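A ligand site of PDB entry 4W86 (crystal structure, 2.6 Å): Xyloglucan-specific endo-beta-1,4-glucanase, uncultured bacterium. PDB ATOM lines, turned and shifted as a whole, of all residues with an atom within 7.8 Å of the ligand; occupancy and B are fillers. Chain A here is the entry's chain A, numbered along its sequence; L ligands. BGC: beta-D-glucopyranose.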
ATOM      1  N   ASN A 148     -14.478  20.311   6.809  1.00  0.00           N
ATOM      2  CA  ASN A 148     -13.091  19.932   6.568  1.00  0.00           C
ATOM      3  C   ASN A 148     -12.519  20.551   5.294  1.00  0.00           C
ATOM      4  O   ASN A 148     -13.007  20.301   4.187  1.00  0.00           O
ATOM      5  CB  ASN A 148     -12.915  18.428   6.487  1.00  0.00           C
ATOM      6  CG  ASN A 148     -11.459  18.019   6.441  1.00  0.00           C
ATOM      7  OD1 ASN A 148     -10.724  18.219   7.403  1.00  0.00           O
ATOM      8  ND2 ASN A 148     -11.027  17.474   5.312  1.00  0.00           N
ATOM      9  N   GLU A 149     -11.453  21.331   5.487  1.00  0.00           N
ATOM     10  CA  GLU A 149     -10.765  22.049   4.415  1.00  0.00           C
ATOM     11  C   GLU A 149     -11.717  22.596   3.350  1.00  0.00           C
ATOM     12  O   GLU A 149     -11.588  22.254   2.179  1.00  0.00           O
ATOM     13  CB  GLU A 149      -9.718  21.132   3.783  1.00  0.00           C
ATOM     14  CG  GLU A 149      -8.644  20.697   4.757  1.00  0.00           C
ATOM     15  CD  GLU A 149      -7.637  19.729   4.154  1.00  0.00           C
ATOM     16  OE1 GLU A 149      -7.925  19.167   3.074  1.00  0.00           O
ATOM     17  OE2 GLU A 149      -6.578  19.529   4.774  1.00  0.00           O
ATOM     18  N   ARG A 151     -13.190  24.572   0.512  1.00  0.00           N
ATOM     19  CA  ARG A 151     -12.490  25.248  -0.575  1.00  0.00           C
ATOM     20  C   ARG A 151     -13.159  24.951  -1.913  1.00  0.00           C
ATOM     21  O   ARG A 151     -14.093  24.163  -1.994  1.00  0.00           O
ATOM     22  CB  ARG A 151     -11.031  24.775  -0.632  1.00  0.00           C
ATOM     23  CG  ARG A 151     -10.886  23.339  -1.121  1.00  0.00           C
ATOM     24  CD  ARG A 151      -9.629  22.671  -0.590  1.00  0.00           C
ATOM     25  NE  ARG A 151      -9.469  21.330  -1.165  1.00  0.00           N
ATOM     26  CZ  ARG A 151     -10.145  20.249  -0.785  1.00  0.00           C
ATOM     27  NH1 ARG A 151     -11.064  20.299   0.171  1.00  0.00           N
ATOM     28  NH2 ARG A 151      -9.904  19.081  -1.385  1.00  0.00           N
ATOM     29  N   GLU A 158      -6.536  27.257  -4.088  1.00  0.00           N
ATOM     30  CA  GLU A 158      -7.172  26.182  -3.319  1.00  0.00           C
ATOM     31  C   GLU A 158      -6.417  25.896  -2.012  1.00  0.00           C
ATOM     32  O   GLU A 158      -7.039  25.783  -0.957  1.00  0.00           O
ATOM     33  CB  GLU A 158      -7.258  24.903  -4.158  1.00  0.00           C
ATOM     34  CG  GLU A 158      -7.830  23.701  -3.425  1.00  0.00           C
ATOM     35  CD  GLU A 158      -7.865  22.445  -4.272  1.00  0.00           C
ATOM     36  OE1 GLU A 158      -7.442  22.490  -5.449  1.00  0.00           O
ATOM     37  OE2 GLU A 158      -8.334  21.405  -3.760  1.00  0.00           O
ATOM     38  N   TRP A 159      -5.101  25.782  -2.117  1.00  0.00           N
ATOM     39  CA  TRP A 159      -4.256  25.430  -0.967  1.00  0.00           C
ATOM     40  C   TRP A 159      -3.455  26.613  -0.405  1.00  0.00           C
ATOM     41  O   TRP A 159      -2.497  26.408   0.339  1.00  0.00           O
ATOM     42  CB  TRP A 159      -3.325  24.282  -1.348  1.00  0.00           C
ATOM     43  CG  TRP A 159      -4.080  23.049  -1.720  1.00  0.00           C
ATOM     44  CD1 TRP A 159      -4.084  22.424  -2.931  1.00  0.00           C
ATOM     45  CD2 TRP A 159      -4.948  22.298  -0.875  1.00  0.00           C
ATOM     46  NE1 TRP A 159      -4.900  21.319  -2.885  1.00  0.00           N
ATOM     47  CE2 TRP A 159      -5.446  21.213  -1.633  1.00  0.00           C
ATOM     48  CE3 TRP A 159      -5.364  22.424   0.463  1.00  0.00           C
ATOM     49  CZ2 TRP A 159      -6.330  20.278  -1.112  1.00  0.00           C
ATOM     50  CZ3 TRP A 159      -6.235  21.489   0.983  1.00  0.00           C
ATOM     51  CH2 TRP A 159      -6.714  20.419   0.196  1.00  0.00           C
ATOM     52  N   SER A 160      -3.852  27.836  -0.746  1.00  0.00           N
ATOM     53  CA  SER A 160      -3.189  29.032  -0.219  1.00  0.00           C
ATOM     54  C   SER A 160      -4.220  30.020   0.350  1.00  0.00           C
ATOM     55  O   SER A 160      -4.045  31.240   0.253  1.00  0.00           O
ATOM     56  CB  SER A 160      -2.334  29.684  -1.307  1.00  0.00           C
ATOM     57  OG  SER A 160      -3.132  30.150  -2.381  1.00  0.00           O
ATOM     58  N   TYR A 198     -10.446  28.917   5.500  1.00  0.00           N
ATOM     59  CA  TYR A 198     -10.483  28.376   4.150  1.00  0.00           C
ATOM     60  C   TYR A 198      -9.391  27.316   3.995  1.00  0.00           C
ATOM     61  O   TYR A 198      -8.210  27.607   4.206  1.00  0.00           O
ATOM     62  CB  TYR A 198     -10.284  29.503   3.120  1.00  0.00           C
ATOM     63  CG  TYR A 198     -10.434  29.067   1.678  1.00  0.00           C
ATOM     64  CD1 TYR A 198      -9.389  28.456   1.000  1.00  0.00           C
ATOM     65  CD2 TYR A 198     -11.621  29.291   0.983  1.00  0.00           C
ATOM     66  CE1 TYR A 198      -9.519  28.061  -0.325  1.00  0.00           C
ATOM     67  CE2 TYR A 198     -11.758  28.904  -0.339  1.00  0.00           C
ATOM     68  CZ  TYR A 198     -10.703  28.290  -0.987  1.00  0.00           C
ATOM     69  OH  TYR A 198     -10.839  27.899  -2.299  1.00  0.00           O
ATOM     70  N   GLY A 199      -9.788  26.097   3.648  1.00  0.00           N
ATOM     71  CA  GLY A 199      -8.856  24.995   3.473  1.00  0.00           C
ATOM     72  C   GLY A 199      -8.031  24.629   4.715  1.00  0.00           C
ATOM     73  O   GLY A 199      -6.995  23.978   4.595  1.00  0.00           O
ATOM     74  N   HIS A 200      -8.513  25.036   5.888  1.00  0.00           N
ATOM     75  CA  HIS A 200      -7.738  24.912   7.129  1.00  0.00           C
ATOM     76  C   HIS A 200      -6.326  25.525   6.993  1.00  0.00           C
ATOM     77  O   HIS A 200      -5.384  25.096   7.653  1.00  0.00           O
ATOM     78  CB  HIS A 200      -7.649  23.449   7.578  1.00  0.00           C
ATOM     79  CG  HIS A 200      -8.818  22.988   8.388  1.00  0.00           C
ATOM     80  ND1 HIS A 200     -10.100  22.940   7.886  1.00  0.00           N
ATOM     81  CD2 HIS A 200      -8.901  22.560   9.670  1.00  0.00           C
ATOM     82  CE1 HIS A 200     -10.915  22.493   8.816  1.00  0.00           C
ATOM     83  NE2 HIS A 200     -10.215  22.257   9.911  1.00  0.00           N
ATOM     84  N   ASN A 201      -6.218  26.546   6.148  1.00  0.00           N
ATOM     85  CA  ASN A 201      -4.933  27.197   5.877  1.00  0.00           C
ATOM     86  C   ASN A 201      -4.616  28.195   6.982  1.00  0.00           C
ATOM     87  O   ASN A 201      -5.503  28.858   7.516  1.00  0.00           O
ATOM     88  CB  ASN A 201      -4.987  27.893   4.505  1.00  0.00           C
ATOM     89  CG  ASN A 201      -3.706  28.625   4.166  1.00  0.00           C
ATOM     90  OD1 ASN A 201      -3.497  29.750   4.583  1.00  0.00           O
ATOM     91  ND2 ASN A 201      -2.842  27.980   3.398  1.00  0.00           N
ATOM     92  N   SER A 202      -3.334  28.293   7.332  1.00  0.00           N
ATOM     93  CA  SER A 202      -2.884  29.121   8.454  1.00  0.00           C
ATOM     94  C   SER A 202      -1.920  30.230   8.047  1.00  0.00           C
ATOM     95  O   SER A 202      -1.055  30.630   8.830  1.00  0.00           O
ATOM     96  CB  SER A 202      -2.241  28.236   9.519  1.00  0.00           C
ATOM     97  OG  SER A 202      -1.017  27.695   9.049  1.00  0.00           O
ATOM     98  N   LEU A 222      -7.058  24.355  12.572  1.00  0.00           N
ATOM     99  CA  LEU A 222      -6.133  24.531  11.468  1.00  0.00           C
ATOM    100  C   LEU A 222      -5.471  23.202  11.147  1.00  0.00           C
ATOM    101  O   LEU A 222      -5.456  22.288  11.984  1.00  0.00           O
ATOM    102  CB  LEU A 222      -5.065  25.562  11.829  1.00  0.00           C
ATOM    103  CG  LEU A 222      -5.579  26.962  12.181  1.00  0.00           C
ATOM    104  CD1 LEU A 222      -4.472  27.804  12.772  1.00  0.00           C
ATOM    105  CD2 LEU A 222      -6.192  27.660  10.977  1.00  0.00           C
ATOM    106  N   HIS A 223      -4.949  23.080   9.938  1.00  0.00           N
ATOM    107  CA  HIS A 223      -4.146  21.929   9.547  1.00  0.00           C
ATOM    108  C   HIS A 223      -2.749  22.415   9.232  1.00  0.00           C
ATOM    109  O   HIS A 223      -2.558  23.305   8.410  1.00  0.00           O
ATOM    110  CB  HIS A 223      -4.737  21.222   8.330  1.00  0.00           C
ATOM    111  CG  HIS A 223      -6.022  20.522   8.617  1.00  0.00           C
ATOM    112  ND1 HIS A 223      -6.820  20.003   7.618  1.00  0.00           N
ATOM    113  CD2 HIS A 223      -6.659  20.263   9.783  1.00  0.00           C
ATOM    114  CE1 HIS A 223      -7.890  19.443   8.164  1.00  0.00           C
ATOM    115  NE2 HIS A 223      -7.818  19.586   9.474  1.00  0.00           N
ATOM    116  N   THR A 224      -1.772  21.832   9.923  1.00  0.00           N
ATOM    117  CA  THR A 224      -0.395  22.270   9.784  1.00  0.00           C
ATOM    118  C   THR A 224       0.528  21.069   9.683  1.00  0.00           C
ATOM    119  O   THR A 224       1.133  20.629  10.666  1.00  0.00           O
ATOM    120  CB  THR A 224       0.012  23.181  10.958  1.00  0.00           C
ATOM    121  OG1 THR A 224      -0.385  22.586  12.193  1.00  0.00           O
ATOM    122  CG2 THR A 224      -0.658  24.546  10.827  1.00  0.00           C
ATOM    123  N   TYR A 225       0.611  20.511   8.475  1.00  0.00           N
ATOM    124  CA  TYR A 225       1.602  19.514   8.149  1.00  0.00           C
ATOM    125  C   TYR A 225       2.873  20.265   7.776  1.00  0.00           C
ATOM    126  O   TYR A 225       3.325  20.223   6.631  1.00  0.00           O
ATOM    127  CB  TYR A 225       1.152  18.657   6.955  1.00  0.00           C
ATOM    128  CG  TYR A 225      -0.096  17.824   7.162  1.00  0.00           C
ATOM    129  CD1 TYR A 225      -1.363  18.393   7.117  1.00  0.00           C
ATOM    130  CD2 TYR A 225      -0.003  16.448   7.343  1.00  0.00           C
ATOM    131  CE1 TYR A 225      -2.507  17.623   7.272  1.00  0.00           C
ATOM    132  CE2 TYR A 225      -1.140  15.668   7.504  1.00  0.00           C
ATOM    133  CZ  TYR A 225      -2.384  16.270   7.468  1.00  0.00           C
ATOM    134  OH  TYR A 225      -3.508  15.493   7.619  1.00  0.00           O
ATOM    135  N   TYR A 228       5.652  21.497   4.663  1.00  0.00           N
ATOM    136  CA  TYR A 228       5.001  20.659   3.652  1.00  0.00           C
ATOM    137  C   TYR A 228       5.980  19.691   2.988  1.00  0.00           C
ATOM    138  O   TYR A 228       5.663  18.517   2.786  1.00  0.00           O
ATOM    139  CB  TYR A 228       4.322  21.523   2.594  1.00  0.00           C
ATOM    140  CG  TYR A 228       3.702  20.739   1.459  1.00  0.00           C
ATOM    141  CD1 TYR A 228       2.563  19.966   1.666  1.00  0.00           C
ATOM    142  CD2 TYR A 228       4.256  20.751   0.176  1.00  0.00           C
ATOM    143  CE1 TYR A 228       1.991  19.227   0.638  1.00  0.00           C
ATOM    144  CE2 TYR A 228       3.690  20.021  -0.861  1.00  0.00           C
ATOM    145  CZ  TYR A 228       2.562  19.259  -0.619  1.00  0.00           C
ATOM    146  OH  TYR A 228       1.991  18.532  -1.644  1.00  0.00           O
ATOM    147  N   THR A 231       6.786  16.728   5.274  1.00  0.00           N
ATOM    148  CA  THR A 231       5.653  15.886   5.627  1.00  0.00           C
ATOM    149  C   THR A 231       5.036  15.140   4.442  1.00  0.00           C
ATOM    150  O   THR A 231       4.530  14.023   4.604  1.00  0.00           O
ATOM    151  CB  THR A 231       4.550  16.715   6.308  1.00  0.00           C
ATOM    152  OG1 THR A 231       4.214  17.828   5.471  1.00  0.00           O
ATOM    153  CG2 THR A 231       5.041  17.230   7.651  1.00  0.00           C
ATOM    154  N   TYR A 232       5.063  15.762   3.260  1.00  0.00           N
ATOM    155  CA  TYR A 232       4.483  15.165   2.047  1.00  0.00           C
ATOM    156  C   TYR A 232       5.550  14.760   1.033  1.00  0.00           C
ATOM    157  O   TYR A 232       6.694  15.215   1.112  1.00  0.00           O
ATOM    158  CB  TYR A 232       3.507  16.156   1.385  1.00  0.00           C
ATOM    159  CG  TYR A 232       2.107  16.120   1.966  1.00  0.00           C
ATOM    160  CD1 TYR A 232       1.805  16.760   3.168  1.00  0.00           C
ATOM    161  CD2 TYR A 232       1.083  15.444   1.306  1.00  0.00           C
ATOM    162  CE1 TYR A 232       0.527  16.719   3.694  1.00  0.00           C
ATOM    163  CE2 TYR A 232      -0.210  15.407   1.824  1.00  0.00           C
ATOM    164  CZ  TYR A 232      -0.477  16.055   3.015  1.00  0.00           C
ATOM    165  OH  TYR A 232      -1.749  16.011   3.528  1.00  0.00           O
ATOM    166  N   GLU A 271      -5.609  18.257  12.174  1.00  0.00           N
ATOM    167  CA  GLU A 271      -4.797  17.323  11.389  1.00  0.00           C
ATOM    168  C   GLU A 271      -3.345  17.776  11.280  1.00  0.00           C
ATOM    169  O   GLU A 271      -3.056  18.954  11.063  1.00  0.00           O
ATOM    170  CB  GLU A 271      -5.322  17.157   9.964  1.00  0.00           C
ATOM    171  CG  GLU A 271      -6.677  16.479   9.831  1.00  0.00           C
ATOM    172  CD  GLU A 271      -7.111  16.336   8.385  1.00  0.00           C
ATOM    173  OE1 GLU A 271      -6.278  16.573   7.479  1.00  0.00           O
ATOM    174  OE2 GLU A 271      -8.284  15.984   8.132  1.00  0.00           O
ATOM    175  N   GLN A 275       4.474  11.839   6.517  1.00  0.00           N
ATOM    176  CA  GLN A 275       4.458  10.578   5.794  1.00  0.00           C
ATOM    177  C   GLN A 275       5.744   9.830   6.064  1.00  0.00           C
ATOM    178  O   GLN A 275       6.823  10.431   6.165  1.00  0.00           O
ATOM    179  CB  GLN A 275       4.279  10.817   4.293  1.00  0.00           C
ATOM    180  CG  GLN A 275       2.927  11.374   3.913  1.00  0.00           C
ATOM    181  CD  GLN A 275       2.760  11.537   2.418  1.00  0.00           C
ATOM    182  OE1 GLN A 275       3.278  10.738   1.640  1.00  0.00           O
ATOM    183  NE2 GLN A 275       2.016  12.557   2.009  1.00  0.00           N
ATOM    184  N   GLU A 314      -0.290   7.778   0.444  1.00  0.00           N
ATOM    185  CA  GLU A 314       0.325   8.646   1.437  1.00  0.00           C
ATOM    186  C   GLU A 314       0.516   7.830   2.715  1.00  0.00           C
ATOM    187  O   GLU A 314      -0.464   7.346   3.288  1.00  0.00           O
ATOM    188  CB  GLU A 314      -0.558   9.870   1.712  1.00  0.00           C
ATOM    189  CG  GLU A 314      -0.816  10.762   0.508  1.00  0.00           C
ATOM    190  CD  GLU A 314      -1.794  11.892   0.792  1.00  0.00           C
ATOM    191  OE1 GLU A 314      -2.424  11.904   1.879  1.00  0.00           O
ATOM    192  OE2 GLU A 314      -1.948  12.772  -0.076  1.00  0.00           O
ATOM    193  N   PHE A 316       0.736   7.788   5.980  1.00  0.00           N
ATOM    194  CA  PHE A 316       0.443   8.410   7.281  1.00  0.00           C
ATOM    195  C   PHE A 316       0.073   7.378   8.347  1.00  0.00           C
ATOM    196  O   PHE A 316      -0.170   7.745   9.506  1.00  0.00           O
ATOM    197  CB  PHE A 316      -0.687   9.427   7.139  1.00  0.00           C
ATOM    198  CG  PHE A 316      -0.270  10.733   6.529  1.00  0.00           C
ATOM    199  CD1 PHE A 316       0.571  11.597   7.215  1.00  0.00           C
ATOM    200  CD2 PHE A 316      -0.746  11.116   5.283  1.00  0.00           C
ATOM    201  CE1 PHE A 316       0.948  12.812   6.664  1.00  0.00           C
ATOM    202  CE2 PHE A 316      -0.376  12.324   4.730  1.00  0.00           C
ATOM    203  CZ  PHE A 316       0.471  13.179   5.422  1.00  0.00           C
HETATM  204  C2  BGC L   1      -1.788  19.831   0.569  1.00  0.00           C
HETATM  205  C3  BGC L   1      -3.097  19.148   0.969  1.00  0.00           C
HETATM  206  C4  BGC L   1      -3.238  19.087   2.484  1.00  0.00           C
HETATM  207  C5  BGC L   1      -2.865  20.437   3.120  1.00  0.00           C
HETATM  208  C6  BGC L   1      -3.472  20.888   4.456  1.00  0.00           C
HETATM  209  C1  BGC L   1      -1.692  21.221   1.200  1.00  0.00           C
HETATM  210  O1  BGC L   1      -0.501  21.893   0.765  1.00  0.00           O
HETATM  211  O2  BGC L   1      -1.716  19.922  -0.867  1.00  0.00           O
HETATM  212  O3  BGC L   1      -3.118  17.821   0.425  1.00  0.00           O
HETATM  213  O4  BGC L   1      -4.580  18.717   2.822  1.00  0.00           O
HETATM  214  O5  BGC L   1      -1.681  21.084   2.624  1.00  0.00           O
HETATM  215  O6  BGC L   1      -4.461  21.902   4.226  1.00  0.00           O
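The side-chain carboxylate of Glu 149 is in hydrogen-bond range of a ring nitrogen (ND1) of His 223 (2.9 Å).
The backbone NH (N) of Glu 149 lies within hydrogen-bond range of a ring nitrogen (ND1) of His 200 (3.2 Å).
NH1 of Arg 151 sits at hydrogen-bond distance from O of Glu 149 (2.9 Å).
The side-chain hydroxyl (OG1) of Thr 231 sits at hydrogen-bond distance from the backbone carbonyl oxygen (O) of Tyr 228 (3.1 Å).
The side-chain amide nitrogen (ND2) of Asn 201 sits at hydrogen-bond distance from the backbone carbonyl oxygen (O) of Trp 159.
CZ3 of Trp 159 touches O4 of the ligand (3.7 Å).
Tyr 228 touches the ligand (CE1 to O1, 3.7 Å).
Tyr 232 touches the ligand.
Hydrophobic or aromatic side chains within 4 Å of the ligand: Trp 159 and Tyr 228.
The side-chain carboxylate (OE2) of Glu 149 is in hydrogen-bond range of an oxygen (O4) of the ligand (2.9 Å).
O of Gly 199 lies within hydrogen-bond range of O6 of the ligand (3.3 Å).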
